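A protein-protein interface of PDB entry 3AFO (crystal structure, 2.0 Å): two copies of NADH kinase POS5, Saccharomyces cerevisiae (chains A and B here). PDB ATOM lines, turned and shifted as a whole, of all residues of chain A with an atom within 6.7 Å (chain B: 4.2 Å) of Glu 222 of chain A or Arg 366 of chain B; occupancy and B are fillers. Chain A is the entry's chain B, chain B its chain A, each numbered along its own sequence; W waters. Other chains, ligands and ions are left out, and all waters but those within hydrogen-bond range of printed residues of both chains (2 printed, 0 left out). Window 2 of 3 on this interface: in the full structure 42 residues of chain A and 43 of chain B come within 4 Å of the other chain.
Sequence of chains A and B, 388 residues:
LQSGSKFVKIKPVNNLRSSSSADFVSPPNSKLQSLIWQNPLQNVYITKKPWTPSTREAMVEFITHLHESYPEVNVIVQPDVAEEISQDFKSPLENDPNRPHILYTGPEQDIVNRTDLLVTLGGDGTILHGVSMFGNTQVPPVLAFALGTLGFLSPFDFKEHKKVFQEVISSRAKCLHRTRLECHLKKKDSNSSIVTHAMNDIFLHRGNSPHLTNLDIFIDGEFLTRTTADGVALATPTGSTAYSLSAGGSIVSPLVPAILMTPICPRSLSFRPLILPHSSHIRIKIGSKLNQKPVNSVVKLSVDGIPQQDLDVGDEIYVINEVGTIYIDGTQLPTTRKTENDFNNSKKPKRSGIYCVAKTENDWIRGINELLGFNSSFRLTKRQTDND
The side-chain amide nitrogen of Asn 362 of chain B lies close to the side-chain carboxylate of Glu 222 of chain A, 3.5 Å away. NH1 of Arg 366 of chain B lies within salt-bridge range of OE1 of Glu 222 of chain A. The backbone carbonyl oxygen of Leu 224 of chain A is in hydrogen-bond range of the side-chain amide nitrogen of Asn 369 of chain B (3.0 Å).
OG1 of Thr 360 of chain B lies within hydrogen-bond range of N of Asn 362 of chain B, 3.1 Å away. The backbone carbonyl oxygen (O) of Ile 365 of chain B lies close to the side-chain amide nitrogen (ND2) of Asn 369 of chain B, at 3.5 Å. O of Ile 217 of chain A is in hydrogen-bond range of N of Leu 224 of chain A.
Water W2 lies within hydrogen-bond range of OG1 of Thr 225 of chain A and OD1 of Asn 369 of chain B. Water W1 lies within hydrogen-bond range of the backbone carbonyl oxygen (O) of Ile 219 of chain A and the side-chain amide oxygen (OD1) of Asn 362 of chain B.
Of the printed residues of chain B, Glu 222 of chain A touches Asn 362 (3.1 Å) and Arg 366 (3.7 Å). Of the printed residues of chain B, Phe 223 of chain A touches Ile 365. Of the printed residues of chain B, Leu 224 of chain A touches Asn 369. Thr 225 of chain A touches none of the printed residues of chain B. Asp 363 of chain B touches none of the printed residues of chain A. Printed residues of chain A within 4 Å of Arg 366 of chain B: Glu 222 (3.7 Å). The nearest printed residue of chain B that does not touch Glu 222 of chain A is Ile 365 of chain B (4.3 Å). The nearest printed residue of chain A that does not touch Arg 366 of chain B is Phe 223 of chain A (6.6 Å).
No position is printed for both chains. Of the 5 pairs that touch across the chains among the printed residues, none has its exchanged pair printed and touching as well.
Hydrophobic or aromatic side chains of chain A that line the printed part of chain B: Ile 219. Of the 10 printed residues of chain B, 4 touch a printed residue of chain A. Among the printed residues, Asp or Glu carboxylates within 4 Å of a Lys or Arg side-chain nitrogen of the other chain: Glu 222 of chain A with Arg 366 of chain B (3.7 Å).
Among the printed residues, pairs that only touch across the chains: Phe 223 of chain A with Ile 365 of chain B (3.6 Å) and Ile 219 of chain A with Ile 365 of chain B (3.8 Å).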
ATOM      1  N   ILE A 217      13.068  -3.547  15.304  1.00  0.00           N
ATOM      2  CA  ILE A 217      13.897  -3.178  14.179  1.00  0.00           C
ATOM      3  C   ILE A 217      14.409  -4.440  13.510  1.00  0.00           C
ATOM      4  O   ILE A 217      14.934  -5.343  14.183  1.00  0.00           O
ATOM      5  CB  ILE A 217      15.089  -2.284  14.627  1.00  0.00           C
ATOM      6  CG1 ILE A 217      14.570  -1.003  15.308  1.00  0.00           C
ATOM      7  CG2 ILE A 217      15.954  -1.957  13.437  1.00  0.00           C
ATOM      8  CD1 ILE A 217      15.668  -0.124  15.981  1.00  0.00           C
ATOM      9  N   PHE A 218      14.238  -4.484  12.188  1.00  0.00           N
ATOM     10  CA  PHE A 218      14.652  -5.616  11.365  1.00  0.00           C
ATOM     11  C   PHE A 218      15.595  -5.140  10.267  1.00  0.00           C
ATOM     12  O   PHE A 218      15.355  -4.112   9.640  1.00  0.00           O
ATOM     13  CB  PHE A 218      13.432  -6.292  10.715  1.00  0.00           C
ATOM     14  CG  PHE A 218      12.489  -6.917  11.695  1.00  0.00           C
ATOM     15  CD1 PHE A 218      12.530  -8.291  11.940  1.00  0.00           C
ATOM     16  CD2 PHE A 218      11.569  -6.140  12.386  1.00  0.00           C
ATOM     17  CE1 PHE A 218      11.666  -8.873  12.872  1.00  0.00           C
ATOM     18  CE2 PHE A 218      10.690  -6.716  13.313  1.00  0.00           C
ATOM     19  CZ  PHE A 218      10.737  -8.078  13.551  1.00  0.00           C
ATOM     20  N   ILE A 219      16.667  -5.890  10.033  1.00  0.00           N
ATOM     21  CA  ILE A 219      17.550  -5.603   8.896  1.00  0.00           C
ATOM     22  C   ILE A 219      17.577  -6.800   7.939  1.00  0.00           C
ATOM     23  O   ILE A 219      17.900  -7.935   8.336  1.00  0.00           O
ATOM     24  CB  ILE A 219      18.985  -5.216   9.344  1.00  0.00           C
ATOM     25  CG1 ILE A 219      18.956  -3.955  10.219  1.00  0.00           C
ATOM     26  CG2 ILE A 219      19.908  -5.002   8.128  1.00  0.00           C
ATOM     27  CD1 ILE A 219      20.174  -3.819  11.134  1.00  0.00           C
ATOM     28  N   ASP A 220      17.238  -6.525   6.682  1.00  0.00           N
ATOM     29  CA  ASP A 220      17.166  -7.551   5.627  1.00  0.00           C
ATOM     30  C   ASP A 220      16.371  -8.777   6.091  1.00  0.00           C
ATOM     31  O   ASP A 220      16.776  -9.913   5.849  1.00  0.00           O
ATOM     32  CB  ASP A 220      18.579  -7.954   5.175  1.00  0.00           C
ATOM     33  CG  ASP A 220      19.391  -6.778   4.653  1.00  0.00           C
ATOM     34  OD1 ASP A 220      18.806  -5.828   4.109  1.00  0.00           O
ATOM     35  OD2 ASP A 220      20.630  -6.815   4.769  1.00  0.00           O
ATOM     36  N   GLY A 221      15.269  -8.540   6.801  1.00  0.00           N
ATOM     37  CA  GLY A 221      14.396  -9.621   7.270  1.00  0.00           C
ATOM     38  C   GLY A 221      14.791 -10.286   8.584  1.00  0.00           C
ATOM     39  O   GLY A 221      14.037 -11.101   9.111  1.00  0.00           O
ATOM     40  N   GLU A 222      15.928  -9.882   9.135  1.00  0.00           N
ATOM     41  CA  GLU A 222      16.433 -10.454  10.371  1.00  0.00           C
ATOM     42  C   GLU A 222      16.262  -9.501  11.545  1.00  0.00           C
ATOM     43  O   GLU A 222      16.641  -8.335  11.452  1.00  0.00           O
ATOM     44  CB  GLU A 222      17.891 -10.812  10.175  1.00  0.00           C
ATOM     45  CG  GLU A 222      18.034 -11.915   9.170  1.00  0.00           C
ATOM     46  CD  GLU A 222      17.536 -13.219   9.729  1.00  0.00           C
ATOM     47  OE1 GLU A 222      18.008 -13.592  10.821  1.00  0.00           O
ATOM     48  OE2 GLU A 222      16.672 -13.858   9.096  1.00  0.00           O
ATOM     49  N   PHE A 223      15.693 -10.000  12.642  1.00  0.00           N
ATOM     50  CA  PHE A 223      15.449  -9.169  13.817  1.00  0.00           C
ATOM     51  C   PHE A 223      16.763  -8.636  14.382  1.00  0.00           C
ATOM     52  O   PHE A 223      17.681  -9.397  14.695  1.00  0.00           O
ATOM     53  CB  PHE A 223      14.651  -9.937  14.881  1.00  0.00           C
ATOM     54  CG  PHE A 223      14.374  -9.142  16.146  1.00  0.00           C
ATOM     55  CD1 PHE A 223      13.491  -8.062  16.143  1.00  0.00           C
ATOM     56  CD2 PHE A 223      14.992  -9.494  17.346  1.00  0.00           C
ATOM     57  CE1 PHE A 223      13.232  -7.335  17.314  1.00  0.00           C
ATOM     58  CE2 PHE A 223      14.733  -8.774  18.521  1.00  0.00           C
ATOM     59  CZ  PHE A 223      13.845  -7.696  18.496  1.00  0.00           C
ATOM     60  N   LEU A 224      16.862  -7.317  14.463  1.00  0.00           N
ATOM     61  CA  LEU A 224      18.024  -6.706  15.101  1.00  0.00           C
ATOM     62  C   LEU A 224      17.794  -6.553  16.599  1.00  0.00           C
ATOM     63  O   LEU A 224      18.553  -7.088  17.399  1.00  0.00           O
ATOM     64  CB  LEU A 224      18.376  -5.344  14.464  1.00  0.00           C
ATOM     65  CG  LEU A 224      19.510  -4.579  15.176  1.00  0.00           C
ATOM     66  CD1 LEU A 224      20.861  -5.255  14.961  1.00  0.00           C
ATOM     67  CD2 LEU A 224      19.567  -3.105  14.759  1.00  0.00           C
ATOM     68  N   THR A 225      16.763  -5.802  16.977  1.00  0.00           N
ATOM     69  CA  THR A 225      16.605  -5.402  18.378  1.00  0.00           C
ATOM     70  C   THR A 225      15.263  -4.733  18.632  1.00  0.00           C
ATOM     71  O   THR A 225      14.613  -4.236  17.704  1.00  0.00           O
ATOM     72  CB  THR A 225      17.770  -4.441  18.823  1.00  0.00           C
ATOM     73  OG1 THR A 225      17.882  -4.423  20.257  1.00  0.00           O
ATOM     74  CG2 THR A 225      17.561  -3.015  18.265  1.00  0.00           C
ATOM     75  N   HIS A 281      17.889  -3.255   3.798  1.00  0.00           N
ATOM     76  CA  HIS A 281      16.453  -3.058   3.927  1.00  0.00           C
ATOM     77  C   HIS A 281      16.132  -3.027   5.413  1.00  0.00           C
ATOM     78  O   HIS A 281      16.351  -3.998   6.125  1.00  0.00           O
ATOM     79  CB  HIS A 281      15.675  -4.176   3.211  1.00  0.00           C
ATOM     80  CG  HIS A 281      15.703  -4.072   1.710  1.00  0.00           C
ATOM     81  ND1 HIS A 281      14.574  -4.229   0.931  1.00  0.00           N
ATOM     82  CD2 HIS A 281      16.721  -3.823   0.848  1.00  0.00           C
ATOM     83  CE1 HIS A 281      14.894  -4.078  -0.344  1.00  0.00           C
ATOM     84  NE2 HIS A 281      16.193  -3.834  -0.422  1.00  0.00           N
ATOM     85  N   THR B 360      26.719 -18.445   8.916  1.00  0.00           N
ATOM     86  CA  THR B 360      25.359 -18.200   8.438  1.00  0.00           C
ATOM     87  C   THR B 360      25.408 -16.941   7.590  1.00  0.00           C
ATOM     88  O   THR B 360      26.462 -16.314   7.473  1.00  0.00           O
ATOM     89  CB  THR B 360      24.355 -17.960   9.617  1.00  0.00           C
ATOM     90  OG1 THR B 360      24.708 -16.756  10.325  1.00  0.00           O
ATOM     91  CG2 THR B 360      24.350 -19.130  10.590  1.00  0.00           C
ATOM     92  N   ASN B 362      23.810 -14.422   8.519  1.00  0.00           N
ATOM     93  CA  ASN B 362      23.505 -13.397   9.508  1.00  0.00           C
ATOM     94  C   ASN B 362      24.459 -13.368  10.708  1.00  0.00           C
ATOM     95  O   ASN B 362      24.047 -13.077  11.841  1.00  0.00           O
ATOM     96  CB  ASN B 362      22.043 -13.550   9.935  1.00  0.00           C
ATOM     97  CG  ASN B 362      21.071 -13.284   8.777  1.00  0.00           C
ATOM     98  OD1 ASN B 362      20.993 -12.163   8.256  1.00  0.00           O
ATOM     99  ND2 ASN B 362      20.342 -14.319   8.364  1.00  0.00           N
ATOM    100  N   ASP B 363      25.735 -13.645  10.440  1.00  0.00           N
ATOM    101  CA  ASP B 363      26.768 -13.734  11.484  1.00  0.00           C
ATOM    102  C   ASP B 363      26.955 -12.412  12.214  1.00  0.00           C
ATOM    103  O   ASP B 363      27.257 -12.392  13.405  1.00  0.00           O
ATOM    104  CB  ASP B 363      28.118 -14.146  10.882  1.00  0.00           C
ATOM    105  CG  ASP B 363      28.197 -15.638  10.547  1.00  0.00           C
ATOM    106  OD1 ASP B 363      27.259 -16.383  10.887  1.00  0.00           O
ATOM    107  OD2 ASP B 363      29.216 -16.058   9.955  1.00  0.00           O
ATOM    108  N   TRP B 364      26.791 -11.317  11.478  1.00  0.00           N
ATOM    109  CA  TRP B 364      27.097  -9.994  11.977  1.00  0.00           C
ATOM    110  C   TRP B 364      26.086  -9.541  13.033  1.00  0.00           C
ATOM    111  O   TRP B 364      26.470  -9.155  14.124  1.00  0.00           O
ATOM    112  CB  TRP B 364      27.182  -8.964  10.838  1.00  0.00           C
ATOM    113  CG  TRP B 364      27.613  -7.609  11.377  1.00  0.00           C
ATOM    114  CD1 TRP B 364      28.823  -7.293  11.935  1.00  0.00           C
ATOM    115  CD2 TRP B 364      26.825  -6.413  11.423  1.00  0.00           C
ATOM    116  NE1 TRP B 364      28.833  -5.966  12.330  1.00  0.00           N
ATOM    117  CE2 TRP B 364      27.624  -5.405  12.012  1.00  0.00           C
ATOM    118  CE3 TRP B 364      25.524  -6.093  11.011  1.00  0.00           C
ATOM    119  CZ2 TRP B 364      27.158  -4.098  12.206  1.00  0.00           C
ATOM    120  CZ3 TRP B 364      25.063  -4.788  11.201  1.00  0.00           C
ATOM    121  CH2 TRP B 364      25.883  -3.810  11.795  1.00  0.00           C
ATOM    122  N   ILE B 365      24.803  -9.591  12.704  1.00  0.00           N
ATOM    123  CA  ILE B 365      23.761  -9.206  13.660  1.00  0.00           C
ATOM    124  C   ILE B 365      23.827 -10.095  14.902  1.00  0.00           C
ATOM    125  O   ILE B 365      23.749  -9.600  16.023  1.00  0.00           O
ATOM    126  CB  ILE B 365      22.348  -9.187  13.015  1.00  0.00           C
ATOM    127  CG1 ILE B 365      22.211  -7.937  12.148  1.00  0.00           C
ATOM    128  CG2 ILE B 365      21.237  -9.235  14.090  1.00  0.00           C
ATOM    129  CD1 ILE B 365      20.904  -7.834  11.384  1.00  0.00           C
ATOM    130  N   ARG B 366      23.999 -11.399  14.696  1.00  0.00           N
ATOM    131  CA  ARG B 366      24.071 -12.340  15.811  1.00  0.00           C
ATOM    132  C   ARG B 366      25.318 -12.121  16.675  1.00  0.00           C
ATOM    133  O   ARG B 366      25.253 -12.234  17.895  1.00  0.00           O
ATOM    134  CB  ARG B 366      23.962 -13.784  15.306  1.00  0.00           C
ATOM    135  CG  ARG B 366      22.601 -14.076  14.699  1.00  0.00           C
ATOM    136  CD  ARG B 366      22.097 -15.467  15.053  1.00  0.00           C
ATOM    137  NE  ARG B 366      22.219 -16.410  13.946  1.00  0.00           N
ATOM    138  CZ  ARG B 366      21.380 -16.465  12.913  1.00  0.00           C
ATOM    139  NH1 ARG B 366      20.363 -15.621  12.832  1.00  0.00           N
ATOM    140  NH2 ARG B 366      21.564 -17.365  11.954  1.00  0.00           N
ATOM    141  N   GLY B 367      26.433 -11.773  16.040  1.00  0.00           N
ATOM    142  CA  GLY B 367      27.679 -11.466  16.751  1.00  0.00           C
ATOM    143  C   GLY B 367      27.584 -10.229  17.639  1.00  0.00           C
ATOM    144  O   GLY B 367      27.955 -10.278  18.817  1.00  0.00           O
ATOM    145  N   ILE B 368      27.090  -9.120  17.088  1.00  0.00           N
ATOM    146  CA  ILE B 368      26.973  -7.890  17.893  1.00  0.00           C
ATOM    147  C   ILE B 368      25.982  -8.076  19.059  1.00  0.00           C
ATOM    148  O   ILE B 368      26.260  -7.641  20.180  1.00  0.00           O
ATOM    149  CB  ILE B 368      26.702  -6.596  17.047  1.00  0.00           C
ATOM    150  CG1 ILE B 368      25.309  -6.596  16.408  1.00  0.00           C
ATOM    151  CG2 ILE B 368      27.798  -6.404  15.988  1.00  0.00           C
ATOM    152  CD1 ILE B 368      24.919  -5.269  15.752  1.00  0.00           C
ATOM    153  N   ASN B 369      24.864  -8.754  18.801  1.00  0.00           N
ATOM    154  CA  ASN B 369      23.888  -9.051  19.857  1.00  0.00           C
ATOM    155  C   ASN B 369      24.416  -9.989  20.932  1.00  0.00           C
ATOM    156  O   ASN B 369      24.365  -9.654  22.112  1.00  0.00           O
ATOM    157  CB  ASN B 369      22.587  -9.623  19.277  1.00  0.00           C
ATOM    158  CG  ASN B 369      21.676  -8.548  18.695  1.00  0.00           C
ATOM    159  OD1 ASN B 369      21.719  -7.380  19.095  1.00  0.00           O
ATOM    160  ND2 ASN B 369      20.827  -8.951  17.758  1.00  0.00           N
ATOM    161  N   GLU B 370      24.922 -11.157  20.526  1.00  0.00           N
ATOM    162  CA  GLU B 370      25.270 -12.216  21.484  1.00  0.00           C
ATOM    163  C   GLU B 370      26.657 -12.101  22.102  1.00  0.00           C
ATOM    164  O   GLU B 370      26.850 -12.455  23.268  1.00  0.00           O
ATOM    165  CB  GLU B 370      25.099 -13.607  20.861  1.00  0.00           C
ATOM    166  CG  GLU B 370      23.679 -13.888  20.377  1.00  0.00           C
ATOM    167  CD  GLU B 370      23.452 -15.344  19.994  1.00  0.00           C
ATOM    168  OE1 GLU B 370      24.392 -16.162  20.118  1.00  0.00           O
ATOM    169  OE2 GLU B 370      22.322 -15.671  19.568  1.00  0.00           O
HETATM  170  O   HOH W   1      20.519  -9.126   8.210  1.00  0.00           O
HETATM  171  O   HOH W   2      19.904  -6.114  20.678  1.00  0.00           O
